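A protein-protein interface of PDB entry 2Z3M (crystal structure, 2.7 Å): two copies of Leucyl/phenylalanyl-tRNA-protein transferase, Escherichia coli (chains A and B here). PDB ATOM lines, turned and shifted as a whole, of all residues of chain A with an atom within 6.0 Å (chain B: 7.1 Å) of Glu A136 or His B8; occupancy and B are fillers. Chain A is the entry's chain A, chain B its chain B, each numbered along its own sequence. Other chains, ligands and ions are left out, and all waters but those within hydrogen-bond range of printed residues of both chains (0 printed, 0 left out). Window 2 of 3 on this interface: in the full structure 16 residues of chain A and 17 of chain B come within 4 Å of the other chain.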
ATOM      1  N   PRO A  85     -13.977  15.495   6.573  1.00  0.00           N
ATOM      2  CA  PRO A  85     -13.998  14.078   6.227  1.00  0.00           C
ATOM      3  C   PRO A  85     -14.346  13.936   4.745  1.00  0.00           C
ATOM      4  O   PRO A  85     -14.643  12.842   4.274  1.00  0.00           O
ATOM      5  CB  PRO A  85     -15.119  13.553   7.095  1.00  0.00           C
ATOM      6  CG  PRO A  85     -16.157  14.639   6.890  1.00  0.00           C
ATOM      7  CD  PRO A  85     -15.328  15.932   6.985  1.00  0.00           C
ATOM      8  N   ARG A  87     -13.651  14.833   0.449  1.00  0.00           N
ATOM      9  CA  ARG A  87     -12.693  15.097  -0.606  1.00  0.00           C
ATOM     10  C   ARG A  87     -13.507  15.920  -1.601  1.00  0.00           C
ATOM     11  O   ARG A  87     -14.679  15.616  -1.850  1.00  0.00           O
ATOM     12  CB  ARG A  87     -12.204  13.773  -1.225  1.00  0.00           C
ATOM     13  CG  ARG A  87     -11.416  13.916  -2.524  1.00  0.00           C
ATOM     14  CD  ARG A  87     -10.643  12.648  -2.887  1.00  0.00           C
ATOM     15  NE  ARG A  87      -9.335  12.609  -2.235  1.00  0.00           N
ATOM     16  CZ  ARG A  87      -8.912  11.623  -1.444  1.00  0.00           C
ATOM     17  NH1 ARG A  87      -9.691  10.572  -1.197  1.00  0.00           N
ATOM     18  NH2 ARG A  87      -7.714  11.695  -0.879  1.00  0.00           N
ATOM     19  N   TRP A 134     -16.873  14.134  -2.116  1.00  0.00           N
ATOM     20  CA  TRP A 134     -16.833  12.723  -1.813  1.00  0.00           C
ATOM     21  C   TRP A 134     -16.589  12.426  -0.344  1.00  0.00           C
ATOM     22  O   TRP A 134     -15.841  13.129   0.338  1.00  0.00           O
ATOM     23  CB  TRP A 134     -15.741  12.031  -2.638  1.00  0.00           C
ATOM     24  CG  TRP A 134     -15.709  12.442  -4.081  1.00  0.00           C
ATOM     25  CD1 TRP A 134     -15.068  13.529  -4.612  1.00  0.00           C
ATOM     26  CD2 TRP A 134     -16.354  11.779  -5.178  1.00  0.00           C
ATOM     27  NE1 TRP A 134     -15.271  13.582  -5.971  1.00  0.00           N
ATOM     28  CE2 TRP A 134     -16.057  12.520  -6.346  1.00  0.00           C
ATOM     29  CE3 TRP A 134     -17.157  10.630  -5.289  1.00  0.00           C
ATOM     30  CZ2 TRP A 134     -16.532  12.149  -7.611  1.00  0.00           C
ATOM     31  CZ3 TRP A 134     -17.632  10.260  -6.544  1.00  0.00           C
ATOM     32  CH2 TRP A 134     -17.316  11.020  -7.690  1.00  0.00           C
ATOM     33  N   ARG A 135     -17.256  11.383   0.135  1.00  0.00           N
ATOM     34  CA  ARG A 135     -17.073  10.897   1.492  1.00  0.00           C
ATOM     35  C   ARG A 135     -16.658   9.475   1.179  1.00  0.00           C
ATOM     36  O   ARG A 135     -17.439   8.715   0.624  1.00  0.00           O
ATOM     37  CB  ARG A 135     -18.385  10.922   2.290  1.00  0.00           C
ATOM     38  CG  ARG A 135     -18.273  10.309   3.683  1.00  0.00           C
ATOM     39  CD  ARG A 135     -17.006  10.760   4.390  1.00  0.00           C
ATOM     40  NE  ARG A 135     -16.794  10.026   5.637  1.00  0.00           N
ATOM     41  CZ  ARG A 135     -15.620   9.901   6.254  1.00  0.00           C
ATOM     42  NH1 ARG A 135     -14.533  10.463   5.742  1.00  0.00           N
ATOM     43  NH2 ARG A 135     -15.532   9.213   7.389  1.00  0.00           N
ATOM     44  N   GLU A 136     -15.422   9.122   1.499  1.00  0.00           N
ATOM     45  CA  GLU A 136     -14.936   7.791   1.186  1.00  0.00           C
ATOM     46  C   GLU A 136     -15.119   7.586  -0.326  1.00  0.00           C
ATOM     47  O   GLU A 136     -14.661   8.403  -1.123  1.00  0.00           O
ATOM     48  CB  GLU A 136     -15.710   6.739   1.986  1.00  0.00           C
ATOM     49  CG  GLU A 136     -15.693   6.979   3.496  1.00  0.00           C
ATOM     50  CD  GLU A 136     -16.227   5.800   4.304  1.00  0.00           C
ATOM     51  OE1 GLU A 136     -17.210   5.155   3.864  1.00  0.00           O
ATOM     52  OE2 GLU A 136     -15.668   5.530   5.393  1.00  0.00           O
ATOM     53  N   ASP A 137     -15.806   6.521  -0.724  1.00  0.00           N
ATOM     54  CA  ASP A 137     -16.014   6.231  -2.141  1.00  0.00           C
ATOM     55  C   ASP A 137     -17.367   6.697  -2.666  1.00  0.00           C
ATOM     56  O   ASP A 137     -17.764   6.333  -3.773  1.00  0.00           O
ATOM     57  CB  ASP A 137     -15.863   4.722  -2.382  1.00  0.00           C
ATOM     58  CG  ASP A 137     -16.877   3.882  -1.586  1.00  0.00           C
ATOM     59  OD1 ASP A 137     -17.364   4.335  -0.526  1.00  0.00           O
ATOM     60  OD2 ASP A 137     -17.175   2.745  -2.015  1.00  0.00           O
ATOM     61  N   GLU A 138     -18.063   7.519  -1.884  1.00  0.00           N
ATOM     62  CA  GLU A 138     -19.389   8.007  -2.259  1.00  0.00           C
ATOM     63  C   GLU A 138     -19.552   9.493  -2.577  1.00  0.00           C
ATOM     64  O   GLU A 138     -18.972  10.362  -1.917  1.00  0.00           O
ATOM     65  CB  GLU A 138     -20.384   7.632  -1.171  1.00  0.00           C
ATOM     66  CG  GLU A 138     -20.987   6.279  -1.385  1.00  0.00           C
ATOM     67  CD  GLU A 138     -22.170   6.338  -2.313  1.00  0.00           C
ATOM     68  OE1 GLU A 138     -22.563   5.279  -2.845  1.00  0.00           O
ATOM     69  OE2 GLU A 138     -22.712   7.449  -2.499  1.00  0.00           O
ATOM     70  N   LEU B   5      -6.696  -2.090  -0.380  1.00  0.00           N
ATOM     71  CA  LEU B   5      -7.631  -0.986  -0.493  1.00  0.00           C
ATOM     72  C   LEU B   5      -8.971  -1.372   0.140  1.00  0.00           C
ATOM     73  O   LEU B   5      -9.214  -2.547   0.429  1.00  0.00           O
ATOM     74  CB  LEU B   5      -7.794  -0.595  -1.967  1.00  0.00           C
ATOM     75  CG  LEU B   5      -6.476  -0.199  -2.654  1.00  0.00           C
ATOM     76  CD1 LEU B   5      -6.732   0.137  -4.116  1.00  0.00           C
ATOM     77  CD2 LEU B   5      -5.843   0.983  -1.928  1.00  0.00           C
ATOM     78  N   SER B   6      -9.824  -0.376   0.367  1.00  0.00           N
ATOM     79  CA  SER B   6     -11.127  -0.589   0.983  1.00  0.00           C
ATOM     80  C   SER B   6     -12.071   0.527   0.578  1.00  0.00           C
ATOM     81  O   SER B   6     -11.657   1.497  -0.047  1.00  0.00           O
ATOM     82  CB  SER B   6     -10.993  -0.596   2.509  1.00  0.00           C
ATOM     83  OG  SER B   6     -10.655   0.691   3.009  1.00  0.00           O
ATOM     84  N   ARG B   7     -13.338   0.404   0.951  1.00  0.00           N
ATOM     85  CA  ARG B   7     -14.323   1.426   0.616  1.00  0.00           C
ATOM     86  C   ARG B   7     -14.084   2.721   1.406  1.00  0.00           C
ATOM     87  O   ARG B   7     -14.659   3.761   1.094  1.00  0.00           O
ATOM     88  CB  ARG B   7     -15.729   0.915   0.930  1.00  0.00           C
ATOM     89  CG  ARG B   7     -15.980   0.734   2.427  1.00  0.00           C
ATOM     90  CD  ARG B   7     -17.462   0.694   2.752  1.00  0.00           C
ATOM     91  NE  ARG B   7     -17.692   0.804   4.191  1.00  0.00           N
ATOM     92  CZ  ARG B   7     -17.527  -0.190   5.062  1.00  0.00           C
ATOM     93  NH1 ARG B   7     -17.136  -1.390   4.645  1.00  0.00           N
ATOM     94  NH2 ARG B   7     -17.738   0.020   6.358  1.00  0.00           N
ATOM     95  N   HIS B   8     -13.226   2.661   2.419  1.00  0.00           N
ATOM     96  CA  HIS B   8     -12.973   3.822   3.261  1.00  0.00           C
ATOM     97  C   HIS B   8     -12.157   4.941   2.641  1.00  0.00           C
ATOM     98  O   HIS B   8     -12.386   6.108   2.950  1.00  0.00           O
ATOM     99  CB  HIS B   8     -12.341   3.367   4.573  1.00  0.00           C
ATOM    100  CG  HIS B   8     -13.212   2.434   5.360  1.00  0.00           C
ATOM    101  ND1 HIS B   8     -14.373   2.843   5.978  1.00  0.00           N
ATOM    102  CD2 HIS B   8     -13.116   1.101   5.582  1.00  0.00           C
ATOM    103  CE1 HIS B   8     -14.957   1.803   6.547  1.00  0.00           C
ATOM    104  NE2 HIS B   8     -14.215   0.733   6.322  1.00  0.00           N
ATOM    105  N   SER B   9     -11.212   4.609   1.767  1.00  0.00           N
ATOM    106  CA  SER B   9     -10.412   5.654   1.129  1.00  0.00           C
ATOM    107  C   SER B   9     -10.280   5.440  -0.375  1.00  0.00           C
ATOM    108  O   SER B   9     -10.189   4.310  -0.844  1.00  0.00           O
ATOM    109  CB  SER B   9      -9.016   5.730   1.761  1.00  0.00           C
ATOM    110  OG  SER B   9      -8.303   6.867   1.295  1.00  0.00           O
ATOM    111  N   ILE B  10     -10.266   6.539  -1.121  1.00  0.00           N
ATOM    112  CA  ILE B  10     -10.148   6.494  -2.573  1.00  0.00           C
ATOM    113  C   ILE B  10      -8.707   6.742  -3.005  1.00  0.00           C
ATOM    114  O   ILE B  10      -8.328   6.459  -4.143  1.00  0.00           O
ATOM    115  CB  ILE B  10     -11.106   7.536  -3.219  1.00  0.00           C
ATOM    116  CG1 ILE B  10     -12.511   6.948  -3.290  1.00  0.00           C
ATOM    117  CG2 ILE B  10     -10.642   7.936  -4.585  1.00  0.00           C
ATOM    118  CD1 ILE B  10     -12.712   5.652  -4.129  1.00  0.00           C
ATOM    119  N   ALA B  11      -7.903   7.244  -2.072  1.00  0.00           N
ATOM    120  CA  ALA B  11      -6.495   7.545  -2.320  1.00  0.00           C
ATOM    121  C   ALA B  11      -5.640   6.303  -2.623  1.00  0.00           C
ATOM    122  O   ALA B  11      -6.097   5.168  -2.487  1.00  0.00           O
ATOM    123  CB  ALA B  11      -5.919   8.306  -1.119  1.00  0.00           C
ATOM    124  N   ALA B  35     -14.474   7.954  -9.508  1.00  0.00           N
ATOM    125  CA  ALA B  35     -13.548   8.736  -8.716  1.00  0.00           C
ATOM    126  C   ALA B  35     -12.245   7.987  -8.388  1.00  0.00           C
ATOM    127  O   ALA B  35     -11.159   8.562  -8.482  1.00  0.00           O
ATOM    128  CB  ALA B  35     -14.243   9.202  -7.438  1.00  0.00           C
ATOM    129  N   ARG B  36     -12.338   6.713  -8.006  1.00  0.00           N
ATOM    130  CA  ARG B  36     -11.131   5.958  -7.685  1.00  0.00           C
ATOM    131  C   ARG B  36     -10.257   5.763  -8.916  1.00  0.00           C
ATOM    132  O   ARG B  36      -9.032   5.850  -8.834  1.00  0.00           O
ATOM    133  CB  ARG B  36     -11.477   4.606  -7.078  1.00  0.00           C
ATOM    134  CG  ARG B  36     -10.264   3.734  -6.791  1.00  0.00           C
ATOM    135  CD  ARG B  36     -10.655   2.495  -6.000  1.00  0.00           C
ATOM    136  NE  ARG B  36     -10.478   2.717  -4.572  1.00  0.00           N
ATOM    137  CZ  ARG B  36     -11.350   2.350  -3.643  1.00  0.00           C
ATOM    138  NH1 ARG B  36     -12.471   1.739  -3.984  1.00  0.00           N
ATOM    139  NH2 ARG B  36     -11.109   2.607  -2.371  1.00  0.00           N
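A ring nitrogen (ND1) of His B8 is in hydrogen-bond range of the side-chain carboxylate (OE2) of Glu A136, at 3.0 Å.
The backbone carbonyl oxygen (O) of Arg B7 lies close to the backbone NH (N) of Asp A137, 3.5 Å away.
Of the printed residues of chain B, Arg A87 touches Ile B10 and Ala B11.
Of the printed residues of chain B, Trp A134 touches Ala B35.
Arg A135 touches none of the printed residues of chain B.
Of the printed residues of chain B, Asp A137 touches Arg B7 and Ile B10.
Glu A138 touches none of the printed residues of chain B.
Of chain A, only Glu A136 comes within 4 Å of His B8.
Of the printed residues of chain A, Ile B10 touches Arg A87, Glu A136 and Asp A137.
The nearest residue of chain B that does not touch Glu A136 is Ser B9 (4.9 Å).
The nearest residue of chain A that does not touch His B8 is Asp A137 (5.0 Å).
No position is printed for both chains.
Of the 8 pairs that touch across the chains among the printed residues, none has its exchanged pair printed and touching as well.
Among the printed residues, pairs that only touch across the chains: Glu A136 with Arg B7, Glu A136 with Ile B10, Trp A134 with Ala B35, Asp A137 with Ile B10, Arg A87 with Ala B11 and Arg A87 with Ile B10.
Hydrophobic or aromatic side chains of chain B that line the printed part of chain A: His B8, Ile B10, Ala B11 and Ala B35.
Printed residues of chain A that touch a printed residue of chain B: Arg A87, Trp A134, Glu A136 and Asp A137.
Along chain A the printed residues that touch a printed residue of chain B span positions 87 to 137.
Among the printed residues, 8 pairs touch across the chains.
O of Arg A87 is in hydrogen-bond range of N of Trp A134.
OG of Ser B6 sits close to N of His B8, 3.3 Å away.
The side-chain hydroxyl (OG) of Ser B9 lies within hydrogen-bond range of the backbone NH (N) of Ala B11, 3.4 Å away.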
